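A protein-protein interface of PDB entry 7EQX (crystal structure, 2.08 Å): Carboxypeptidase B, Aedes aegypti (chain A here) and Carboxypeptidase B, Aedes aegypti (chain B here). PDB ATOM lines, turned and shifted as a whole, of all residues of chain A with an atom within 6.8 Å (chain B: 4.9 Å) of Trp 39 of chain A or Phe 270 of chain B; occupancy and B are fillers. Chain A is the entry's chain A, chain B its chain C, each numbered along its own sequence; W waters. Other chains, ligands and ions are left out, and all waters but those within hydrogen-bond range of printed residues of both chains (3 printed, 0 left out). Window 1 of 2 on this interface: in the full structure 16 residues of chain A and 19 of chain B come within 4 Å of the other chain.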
ATOM      1  N   TYR A   7      17.247  36.846 -12.503  1.00  0.00           N
ATOM      2  CA  TYR A   7      18.641  36.477 -12.700  1.00  0.00           C
ATOM      3  C   TYR A   7      19.174  36.926 -14.059  1.00  0.00           C
ATOM      4  O   TYR A   7      20.163  36.368 -14.548  1.00  0.00           O
ATOM      5  CB  TYR A   7      18.811  34.971 -12.509  1.00  0.00           C
ATOM      6  CG  TYR A   7      18.880  34.601 -11.049  1.00  0.00           C
ATOM      7  CD1 TYR A   7      19.979  34.959 -10.283  1.00  0.00           C
ATOM      8  CD2 TYR A   7      17.836  33.927 -10.428  1.00  0.00           C
ATOM      9  CE1 TYR A   7      20.054  34.638  -8.948  1.00  0.00           C
ATOM     10  CE2 TYR A   7      17.899  33.601  -9.084  1.00  0.00           C
ATOM     11  CZ  TYR A   7      19.013  33.962  -8.351  1.00  0.00           C
ATOM     12  OH  TYR A   7      19.100  33.647  -7.014  1.00  0.00           O
ATOM     13  N   VAL A  12      27.204  31.764 -14.353  1.00  0.00           N
ATOM     14  CA  VAL A  12      27.855  30.813 -13.461  1.00  0.00           C
ATOM     15  C   VAL A  12      29.190  30.443 -14.084  1.00  0.00           C
ATOM     16  O   VAL A  12      29.258  30.133 -15.279  1.00  0.00           O
ATOM     17  CB  VAL A  12      26.989  29.566 -13.220  1.00  0.00           C
ATOM     18  CG1 VAL A  12      27.662  28.643 -12.216  1.00  0.00           C
ATOM     19  CG2 VAL A  12      25.615  29.972 -12.725  1.00  0.00           C
ATOM     20  N   ARG A  30      35.694  34.167  -1.829  1.00  0.00           N
ATOM     21  CA  ARG A  30      34.376  33.953  -1.242  1.00  0.00           C
ATOM     22  C   ARG A  30      34.230  34.709   0.075  1.00  0.00           C
ATOM     23  O   ARG A  30      33.222  35.384   0.309  1.00  0.00           O
ATOM     24  CB  ARG A  30      34.124  32.459  -1.032  1.00  0.00           C
ATOM     25  CG  ARG A  30      32.727  32.150  -0.517  1.00  0.00           C
ATOM     26  CD  ARG A  30      32.497  30.655  -0.362  1.00  0.00           C
ATOM     27  NE  ARG A  30      33.173  30.101   0.805  1.00  0.00           N
ATOM     28  CZ  ARG A  30      32.999  28.865   1.252  1.00  0.00           C
ATOM     29  NH1 ARG A  30      32.170  28.023   0.655  1.00  0.00           N
ATOM     30  NH2 ARG A  30      33.671  28.462   2.326  1.00  0.00           N
ATOM     31  N   ASP A  37      27.923  34.494  -5.063  1.00  0.00           N
ATOM     32  CA  ASP A  37      27.205  33.322  -4.563  1.00  0.00           C
ATOM     33  C   ASP A  37      27.973  32.071  -4.989  1.00  0.00           C
ATOM     34  O   ASP A  37      27.780  31.547  -6.087  1.00  0.00           O
ATOM     35  CB  ASP A  37      25.766  33.304  -5.086  1.00  0.00           C
ATOM     36  CG  ASP A  37      24.939  32.169  -4.500  1.00  0.00           C
ATOM     37  OD1 ASP A  37      25.457  31.417  -3.649  1.00  0.00           O
ATOM     38  OD2 ASP A  37      23.761  32.037  -4.887  1.00  0.00           O
ATOM     39  N   PHE A  38      28.844  31.589  -4.104  1.00  0.00           N
ATOM     40  CA  PHE A  38      29.571  30.345  -4.339  1.00  0.00           C
ATOM     41  C   PHE A  38      28.628  29.164  -4.138  1.00  0.00           C
ATOM     42  O   PHE A  38      28.189  28.895  -3.015  1.00  0.00           O
ATOM     43  CB  PHE A  38      30.768  30.240  -3.401  1.00  0.00           C
ATOM     44  CG  PHE A  38      32.001  30.940  -3.902  1.00  0.00           C
ATOM     45  CD1 PHE A  38      32.027  32.319  -4.039  1.00  0.00           C
ATOM     46  CD2 PHE A  38      33.139  30.216  -4.225  1.00  0.00           C
ATOM     47  CE1 PHE A  38      33.166  32.964  -4.500  1.00  0.00           C
ATOM     48  CE2 PHE A  38      34.280  30.853  -4.682  1.00  0.00           C
ATOM     49  CZ  PHE A  38      34.294  32.228  -4.821  1.00  0.00           C
ATOM     50  N   TRP A  39      28.310  28.459  -5.221  1.00  0.00           N
ATOM     51  CA  TRP A  39      27.473  27.269  -5.115  1.00  0.00           C
ATOM     52  C   TRP A  39      28.235  26.074  -4.558  1.00  0.00           C
ATOM     53  O   TRP A  39      27.636  25.215  -3.905  1.00  0.00           O
ATOM     54  CB  TRP A  39      26.887  26.924  -6.483  1.00  0.00           C
ATOM     55  CG  TRP A  39      25.792  27.849  -6.892  1.00  0.00           C
ATOM     56  CD1 TRP A  39      25.275  28.878  -6.159  1.00  0.00           C
ATOM     57  CD2 TRP A  39      25.077  27.841  -8.133  1.00  0.00           C
ATOM     58  NE1 TRP A  39      24.281  29.509  -6.866  1.00  0.00           N
ATOM     59  CE2 TRP A  39      24.137  28.889  -8.079  1.00  0.00           C
ATOM     60  CE3 TRP A  39      25.135  27.045  -9.282  1.00  0.00           C
ATOM     61  CZ2 TRP A  39      23.263  29.166  -9.130  1.00  0.00           C
ATOM     62  CZ3 TRP A  39      24.269  27.325 -10.326  1.00  0.00           C
ATOM     63  CH2 TRP A  39      23.345  28.374 -10.242  1.00  0.00           C
ATOM     64  N   HIS A  40      29.543  26.005  -4.789  1.00  0.00           N
ATOM     65  CA  HIS A  40      30.320  24.826  -4.433  1.00  0.00           C
ATOM     66  C   HIS A  40      31.790  25.214  -4.344  1.00  0.00           C
ATOM     67  O   HIS A  40      32.304  25.887  -5.240  1.00  0.00           O
ATOM     68  CB  HIS A  40      30.109  23.716  -5.474  1.00  0.00           C
ATOM     69  CG  HIS A  40      30.721  22.402  -5.099  1.00  0.00           C
ATOM     70  ND1 HIS A  40      30.095  21.500  -4.264  1.00  0.00           N
ATOM     71  CD2 HIS A  40      31.897  21.834  -5.455  1.00  0.00           C
ATOM     72  CE1 HIS A  40      30.863  20.436  -4.117  1.00  0.00           C
ATOM     73  NE2 HIS A  40      31.963  20.612  -4.829  1.00  0.00           N
ATOM     74  N   LEU A  41      32.454  24.798  -3.267  1.00  0.00           N
ATOM     75  CA  LEU A  41      33.883  25.063  -3.092  1.00  0.00           C
ATOM     76  C   LEU A  41      34.437  24.059  -2.095  1.00  0.00           C
ATOM     77  O   LEU A  41      33.981  24.015  -0.948  1.00  0.00           O
ATOM     78  CB  LEU A  41      34.126  26.492  -2.606  1.00  0.00           C
ATOM     79  CG  LEU A  41      35.564  26.836  -2.196  1.00  0.00           C
ATOM     80  CD1 LEU A  41      36.559  26.461  -3.290  1.00  0.00           C
ATOM     81  CD2 LEU A  41      35.688  28.307  -1.831  1.00  0.00           C
ATOM     82  N   ALA A  49      34.834  24.171  -8.551  1.00  0.00           N
ATOM     83  CA  ALA A  49      34.075  25.202  -7.863  1.00  0.00           C
ATOM     84  C   ALA A  49      33.111  25.874  -8.834  1.00  0.00           C
ATOM     85  O   ALA A  49      33.404  26.033 -10.022  1.00  0.00           O
ATOM     86  CB  ALA A  49      35.011  26.239  -7.247  1.00  0.00           C
ATOM     87  N   ARG A  50      31.943  26.260  -8.325  1.00  0.00           N
ATOM     88  CA  ARG A  50      30.932  26.939  -9.125  1.00  0.00           C
ATOM     89  C   ARG A  50      30.490  28.204  -8.407  1.00  0.00           C
ATOM     90  O   ARG A  50      30.162  28.164  -7.217  1.00  0.00           O
ATOM     91  CB  ARG A  50      29.734  26.028  -9.398  1.00  0.00           C
ATOM     92  CG  ARG A  50      30.091  24.785 -10.200  1.00  0.00           C
ATOM     93  CD  ARG A  50      29.513  24.852 -11.601  1.00  0.00           C
ATOM     94  NE  ARG A  50      30.142  23.891 -12.500  1.00  0.00           N
ATOM     95  CZ  ARG A  50      29.476  23.040 -13.268  1.00  0.00           C
ATOM     96  NH1 ARG A  50      28.155  22.985 -13.254  1.00  0.00           N
ATOM     97  NH2 ARG A  50      30.154  22.221 -14.067  1.00  0.00           N
ATOM     98  N   VAL A  51      30.480  29.322  -9.131  1.00  0.00           N
ATOM     99  CA  VAL A  51      30.184  30.631  -8.558  1.00  0.00           C
ATOM    100  C   VAL A  51      29.155  31.324  -9.437  1.00  0.00           C
ATOM    101  O   VAL A  51      29.374  31.487 -10.643  1.00  0.00           O
ATOM    102  CB  VAL A  51      31.444  31.505  -8.431  1.00  0.00           C
ATOM    103  CG1 VAL A  51      31.112  32.815  -7.726  1.00  0.00           C
ATOM    104  CG2 VAL A  51      32.550  30.759  -7.702  1.00  0.00           C
ATOM    105  N   LEU A  52      28.045  31.744  -8.833  1.00  0.00           N
ATOM    106  CA  LEU A  52      27.043  32.553  -9.506  1.00  0.00           C
ATOM    107  C   LEU A  52      27.375  34.027  -9.295  1.00  0.00           C
ATOM    108  O   LEU A  52      27.546  34.471  -8.154  1.00  0.00           O
ATOM    109  CB  LEU A  52      25.649  32.227  -8.969  1.00  0.00           C
ATOM    110  CG  LEU A  52      24.489  33.127  -9.391  1.00  0.00           C
ATOM    111  CD1 LEU A  52      24.042  32.771 -10.797  1.00  0.00           C
ATOM    112  CD2 LEU A  52      23.333  32.995  -8.413  1.00  0.00           C
ATOM    113  N   ILE A  76      27.335  28.669 -17.398  1.00  0.00           N
ATOM    114  CA  ILE A  76      26.001  29.163 -17.721  1.00  0.00           C
ATOM    115  C   ILE A  76      26.169  30.614 -18.136  1.00  0.00           C
ATOM    116  O   ILE A  76      26.604  31.447 -17.330  1.00  0.00           O
ATOM    117  CB  ILE A  76      25.015  29.035 -16.547  1.00  0.00           C
ATOM    118  CG1 ILE A  76      24.665  27.567 -16.306  1.00  0.00           C
ATOM    119  CG2 ILE A  76      23.751  29.827 -16.831  1.00  0.00           C
ATOM    120  CD1 ILE A  76      24.035  27.309 -14.955  1.00  0.00           C
ATOM    121  N   VAL A  79      21.498  32.925 -16.973  1.00  0.00           N
ATOM    122  CA  VAL A  79      20.536  32.198 -16.149  1.00  0.00           C
ATOM    123  C   VAL A  79      19.116  32.516 -16.601  1.00  0.00           C
ATOM    124  O   VAL A  79      18.191  31.738 -16.339  1.00  0.00           O
ATOM    125  CB  VAL A  79      20.744  32.524 -14.652  1.00  0.00           C
ATOM    126  CG1 VAL A  79      19.882  31.624 -13.778  1.00  0.00           C
ATOM    127  CG2 VAL A  79      22.207  32.374 -14.273  1.00  0.00           C
ATOM    128  N   ARG B  64      18.113  25.956  -0.470  1.00  0.00           N
ATOM    129  CA  ARG B  64      18.201  25.534  -1.864  1.00  0.00           C
ATOM    130  C   ARG B  64      18.607  24.074  -2.040  1.00  0.00           C
ATOM    131  O   ARG B  64      18.590  23.581  -3.174  1.00  0.00           O
ATOM    132  CB  ARG B  64      19.184  26.430  -2.621  1.00  0.00           C
ATOM    133  CG  ARG B  64      20.600  26.411  -2.067  1.00  0.00           C
ATOM    134  CD  ARG B  64      21.427  27.528  -2.684  1.00  0.00           C
ATOM    135  NE  ARG B  64      22.808  27.522  -2.214  1.00  0.00           N
ATOM    136  CZ  ARG B  64      23.679  28.495  -2.443  1.00  0.00           C
ATOM    137  NH1 ARG B  64      23.338  29.583  -3.115  1.00  0.00           N
ATOM    138  NH2 ARG B  64      24.924  28.371  -1.993  1.00  0.00           N
ATOM    139  N   GLU B  65      18.965  23.372  -0.967  1.00  0.00           N
ATOM    140  CA  GLU B  65      19.496  22.008  -1.071  1.00  0.00           C
ATOM    141  C   GLU B  65      18.337  21.006  -1.082  1.00  0.00           C
ATOM    142  O   GLU B  65      18.155  20.186  -0.180  1.00  0.00           O
ATOM    143  CB  GLU B  65      20.490  21.747   0.058  1.00  0.00           C
ATOM    144  CG  GLU B  65      21.796  22.552  -0.084  1.00  0.00           C
ATOM    145  CD  GLU B  65      22.663  22.562   1.181  1.00  0.00           C
ATOM    146  OE1 GLU B  65      22.508  21.683   2.050  1.00  0.00           O
ATOM    147  OE2 GLU B  65      23.530  23.448   1.313  1.00  0.00           O
ATOM    148  N   TRP B  66      17.553  21.079  -2.164  1.00  0.00           N
ATOM    149  CA  TRP B  66      16.249  20.419  -2.219  1.00  0.00           C
ATOM    150  C   TRP B  66      16.338  18.895  -2.161  1.00  0.00           C
ATOM    151  O   TRP B  66      15.380  18.244  -1.731  1.00  0.00           O
ATOM    152  CB  TRP B  66      15.502  20.837  -3.484  1.00  0.00           C
ATOM    153  CG  TRP B  66      14.958  22.233  -3.450  1.00  0.00           C
ATOM    154  CD1 TRP B  66      15.156  23.174  -2.477  1.00  0.00           C
ATOM    155  CD2 TRP B  66      14.118  22.846  -4.436  1.00  0.00           C
ATOM    156  NE1 TRP B  66      14.491  24.336  -2.801  1.00  0.00           N
ATOM    157  CE2 TRP B  66      13.849  24.159  -3.998  1.00  0.00           C
ATOM    158  CE3 TRP B  66      13.572  22.413  -5.648  1.00  0.00           C
ATOM    159  CZ2 TRP B  66      13.053  25.038  -4.727  1.00  0.00           C
ATOM    160  CZ3 TRP B  66      12.782  23.290  -6.372  1.00  0.00           C
ATOM    161  CH2 TRP B  66      12.530  24.585  -5.910  1.00  0.00           C
ATOM    162  N   ILE B  67      17.447  18.299  -2.602  1.00  0.00           N
ATOM    163  CA  ILE B  67      17.496  16.840  -2.627  1.00  0.00           C
ATOM    164  C   ILE B  67      17.605  16.260  -1.222  1.00  0.00           C
ATOM    165  O   ILE B  67      17.327  15.072  -1.021  1.00  0.00           O
ATOM    166  CB  ILE B  67      18.640  16.337  -3.529  1.00  0.00           C
ATOM    167  CG1 ILE B  67      18.380  14.888  -3.959  1.00  0.00           C
ATOM    168  CG2 ILE B  67      19.985  16.445  -2.818  1.00  0.00           C
ATOM    169  CD1 ILE B  67      17.255  14.729  -4.964  1.00  0.00           C
ATOM    170  N   ARG B 114      15.389  30.688  -6.095  1.00  0.00           N
ATOM    171  CA  ARG B 114      15.773  29.278  -6.054  1.00  0.00           C
ATOM    172  C   ARG B 114      17.087  29.045  -5.316  1.00  0.00           C
ATOM    173  O   ARG B 114      17.301  27.951  -4.781  1.00  0.00           O
ATOM    174  CB  ARG B 114      15.877  28.723  -7.481  1.00  0.00           C
ATOM    175  CG  ARG B 114      16.329  27.259  -7.583  1.00  0.00           C
ATOM    176  CD  ARG B 114      15.276  26.322  -7.013  1.00  0.00           C
ATOM    177  NE  ARG B 114      15.674  24.915  -7.024  1.00  0.00           N
ATOM    178  CZ  ARG B 114      16.541  24.366  -6.183  1.00  0.00           C
ATOM    179  NH1 ARG B 114      17.158  25.083  -5.259  1.00  0.00           N
ATOM    180  NH2 ARG B 114      16.790  23.061  -6.268  1.00  0.00           N
ATOM    181  N   PHE B 115      17.964  30.047  -5.250  1.00  0.00           N
ATOM    182  CA  PHE B 115      19.282  29.867  -4.656  1.00  0.00           C
ATOM    183  C   PHE B 115      19.394  30.524  -3.286  1.00  0.00           C
ATOM    184  O   PHE B 115      20.506  30.746  -2.794  1.00  0.00           O
ATOM    185  CB  PHE B 115      20.352  30.394  -5.610  1.00  0.00           C
ATOM    186  CG  PHE B 115      20.157  29.935  -7.024  1.00  0.00           C
ATOM    187  CD1 PHE B 115      20.189  28.585  -7.334  1.00  0.00           C
ATOM    188  CD2 PHE B 115      19.913  30.843  -8.037  1.00  0.00           C
ATOM    189  CE1 PHE B 115      19.995  28.150  -8.631  1.00  0.00           C
ATOM    190  CE2 PHE B 115      19.719  30.416  -9.340  1.00  0.00           C
ATOM    191  CZ  PHE B 115      19.760  29.069  -9.635  1.00  0.00           C
ATOM    192  N   SER B 187      23.538  19.088   0.403  1.00  0.00           N
ATOM    193  CA  SER B 187      23.944  18.906  -0.983  1.00  0.00           C
ATOM    194  C   SER B 187      24.773  20.118  -1.388  1.00  0.00           C
ATOM    195  O   SER B 187      24.598  21.206  -0.833  1.00  0.00           O
ATOM    196  CB  SER B 187      22.723  18.728  -1.902  1.00  0.00           C
ATOM    197  OG  SER B 187      22.166  19.978  -2.271  1.00  0.00           O
ATOM    198  N   TYR B 188      25.682  19.935  -2.347  1.00  0.00           N
ATOM    199  CA  TYR B 188      25.946  18.666  -3.025  1.00  0.00           C
ATOM    200  C   TYR B 188      27.437  18.335  -3.013  1.00  0.00           C
ATOM    201  O   TYR B 188      28.247  19.145  -2.568  1.00  0.00           O
ATOM    202  CB  TYR B 188      25.430  18.719  -4.469  1.00  0.00           C
ATOM    203  CG  TYR B 188      26.172  19.695  -5.361  1.00  0.00           C
ATOM    204  CD1 TYR B 188      25.781  21.026  -5.450  1.00  0.00           C
ATOM    205  CD2 TYR B 188      27.259  19.280  -6.122  1.00  0.00           C
ATOM    206  CE1 TYR B 188      26.458  21.919  -6.267  1.00  0.00           C
ATOM    207  CE2 TYR B 188      27.942  20.162  -6.937  1.00  0.00           C
ATOM    208  CZ  TYR B 188      27.538  21.480  -7.008  1.00  0.00           C
ATOM    209  OH  TYR B 188      28.219  22.354  -7.824  1.00  0.00           O
ATOM    210  N   GLY B 265      22.916  17.564  -9.302  1.00  0.00           N
ATOM    211  CA  GLY B 265      22.228  17.367 -10.565  1.00  0.00           C
ATOM    212  C   GLY B 265      21.679  18.690 -11.045  1.00  0.00           C
ATOM    213  O   GLY B 265      21.592  19.662 -10.290  1.00  0.00           O
ATOM    214  N   ASN B 267      21.576  22.086 -13.706  1.00  0.00           N
ATOM    215  CA  ASN B 267      22.569  23.101 -14.044  1.00  0.00           C
ATOM    216  C   ASN B 267      23.276  23.668 -12.817  1.00  0.00           C
ATOM    217  O   ASN B 267      24.392  24.182 -12.948  1.00  0.00           O
ATOM    218  CB  ASN B 267      21.903  24.233 -14.833  1.00  0.00           C
ATOM    219  CG  ASN B 267      20.786  24.911 -14.056  1.00  0.00           C
ATOM    220  OD1 ASN B 267      19.672  24.392 -13.965  1.00  0.00           O
ATOM    221  ND2 ASN B 267      21.080  26.078 -13.493  1.00  0.00           N
ATOM    222  N   GLY B 268      22.663  23.580 -11.639  1.00  0.00           N
ATOM    223  CA  GLY B 268      23.246  24.160 -10.445  1.00  0.00           C
ATOM    224  C   GLY B 268      23.758  23.177  -9.414  1.00  0.00           C
ATOM    225  O   GLY B 268      24.296  23.585  -8.379  1.00  0.00           O
ATOM    226  N   GLY B 269      23.590  21.887  -9.666  1.00  0.00           N
ATOM    227  CA  GLY B 269      23.931  20.903  -8.640  1.00  0.00           C
ATOM    228  C   GLY B 269      22.870  20.775  -7.564  1.00  0.00           C
ATOM    229  O   GLY B 269      22.487  19.659  -7.200  1.00  0.00           O
ATOM    230  N   PHE B 270      22.389  21.907  -7.037  1.00  0.00           N
ATOM    231  CA  PHE B 270      21.330  21.904  -6.035  1.00  0.00           C
ATOM    232  C   PHE B 270      19.994  21.448  -6.596  1.00  0.00           C
ATOM    233  O   PHE B 270      19.102  21.087  -5.820  1.00  0.00           O
ATOM    234  CB  PHE B 270      21.143  23.303  -5.446  1.00  0.00           C
ATOM    235  CG  PHE B 270      22.344  23.832  -4.743  1.00  0.00           C
ATOM    236  CD1 PHE B 270      22.949  23.110  -3.730  1.00  0.00           C
ATOM    237  CD2 PHE B 270      22.878  25.055  -5.104  1.00  0.00           C
ATOM    238  CE1 PHE B 270      24.059  23.606  -3.081  1.00  0.00           C
ATOM    239  CE2 PHE B 270      23.986  25.551  -4.463  1.00  0.00           C
ATOM    240  CZ  PHE B 270      24.579  24.825  -3.449  1.00  0.00           C
ATOM    241  N   ASN B 271      19.821  21.484  -7.912  1.00  0.00           N
ATOM    242  CA  ASN B 271      18.513  21.316  -8.539  1.00  0.00           C
ATOM    243  C   ASN B 271      18.568  20.206  -9.580  1.00  0.00           C
ATOM    244  O   ASN B 271      18.494  20.467 -10.787  1.00  0.00           O
ATOM    245  CB  ASN B 271      18.039  22.627  -9.170  1.00  0.00           C
ATOM    246  N   PRO B 272      18.697  18.952  -9.151  1.00  0.00           N
ATOM    247  CA  PRO B 272      18.457  17.846 -10.069  1.00  0.00           C
ATOM    248  C   PRO B 272      17.031  17.920 -10.585  1.00  0.00           C
ATOM    249  O   PRO B 272      16.121  18.309  -9.841  1.00  0.00           O
ATOM    250  CB  PRO B 272      18.675  16.598  -9.197  1.00  0.00           C
ATOM    251  CG  PRO B 272      19.494  17.072  -8.044  1.00  0.00           C
ATOM    252  CD  PRO B 272      19.030  18.472  -7.798  1.00  0.00           C
HETATM  253  O   HOH W   1      26.322  31.464  -1.219  1.00  0.00           O
HETATM  254  O   HOH W   2      26.515  25.921  -1.381  1.00  0.00           O
HETATM  255  O   HOH W   3      27.646  22.430  -3.006  1.00  0.00           O
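OD1 of Asp 37 of chain A is in salt-bridge range of NH1 of Arg 64 of chain B (2.9 Å).
The backbone carbonyl oxygen (O) of Phe 38 of chain A sits at hydrogen-bond distance from the guanidinium group (NH2) of Arg 64 of chain B (3.5 Å).
A ring nitrogen (ND1) of His 40 of chain A sits close to the backbone carbonyl oxygen (O) of Tyr 188 of chain B, 3.4 Å away.
The backbone NH of Val 12 of chain A lies within hydrogen-bond range of the backbone carbonyl oxygen of Ile 76 of chain A (3.1 Å).
O of Asp 37 of chain A is in hydrogen-bond range of N of Leu 52 of chain A.
The backbone NH (N) of Trp 39 of chain A sits at hydrogen-bond distance from the backbone carbonyl oxygen (O) of Arg 50 of chain A (2.7 Å).
The backbone NH (N) of Arg 50 of chain A is in hydrogen-bond range of the backbone carbonyl oxygen (O) of His 40 of chain A (3.1 Å).
The guanidinium group (NH1) of Arg 64 of chain B lies within hydrogen-bond range of the backbone carbonyl oxygen (O) of Phe 115 of chain B, 3.1 Å away.
The guanidinium group of Arg 114 of chain B is in hydrogen-bond range of the backbone carbonyl oxygen of Phe 270 of chain B, at 3.1 Å.
Among the printed residues, merely in contact across the chains: Tyr 7 of chain A with Phe 115 of chain B (3.1 Å), Trp 39 of chain A with Phe 270 of chain B (3.1 Å), Trp 39 of chain A with Gly 268 of chain B (3.3 Å), Trp 39 of chain A with Phe 115 of chain B (3.5 Å), Ile 76 of chain A with Asn 267 of chain B (3.5 Å), Trp 39 of chain A with Arg 64 of chain B (3.7 Å), Asp 37 of chain A with Phe 115 of chain B (3.9 Å), Arg 50 of chain A with Tyr 188 of chain B (3.9 Å) and Arg 50 of chain A with Asn 267 of chain B (3.96 Å).
Of chain B, only Arg 64, Phe 115, Gly 268 and Phe 270 come within 4 Å of Trp 39 of chain A.
Phe 270 of chain B touches just one residue of chain A: Trp 39.
Of the printed residues of chain A, Asn 267 of chain B touches Arg 50 (3.96 Å) and Ile 76 (3.5 Å).
Of the printed residues of chain B, His 40 of chain A touches Tyr 188.
Of the printed residues of chain B, Tyr 7 of chain A touches Phe 115.
Printed residues of chain A within 4 Å of Arg 64 of chain B: Asp 37 (2.9 Å), Phe 38 (3.5 Å) and Trp 39 (3.7 Å).
The nearest residue of chain B that does not touch Trp 39 of chain A is Asn 267 of chain B (4.1 Å).
The nearest printed residue of chain B that does not touch Asp 37 of chain A is Phe 270 of chain B (6.1 Å).
Of the 15 printed residues of chain B, 6 touch a printed residue of chain A.
Hydrophobic or aromatic side chains of chain B within 4 Å of the printed part of chain A: Phe 115, Tyr 188 and Phe 270.
Printed residues of chain A that touch a printed residue of chain B: Tyr 7, Asp 37, Phe 38, Trp 39, His 40, Arg 50 and Ile 76.
Hydrophobic or aromatic side chains of chain A within 4 Å of the printed part of chain B: Tyr 7, Trp 39, His 40 and Ile 76.
Among the printed residues, 12 pairs touch across the chains.
Among the printed residues, Asp or Glu carboxylates within 4 Å of a Lys or Arg side-chain nitrogen of the other chain: Asp 37 of chain A with Arg 64 of chain B.
Water W1 bridges the side-chain carboxylate of Asp 37 of chain A (2.6 Å) and the guanidinium group of Arg 64 of chain B (3.5 Å).
Water W2 lies within hydrogen-bond range of the backbone carbonyl oxygen (O) of Trp 39 of chain A and the guanidinium group (NH2) of Arg 64 of chain B.
Water W3 lies within hydrogen-bond range of ND1 of His 40 of chain A (2.9 Å), O of Trp 39 of chain A (2.9 Å) and N of Tyr 188 of chain B (3.2 Å).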
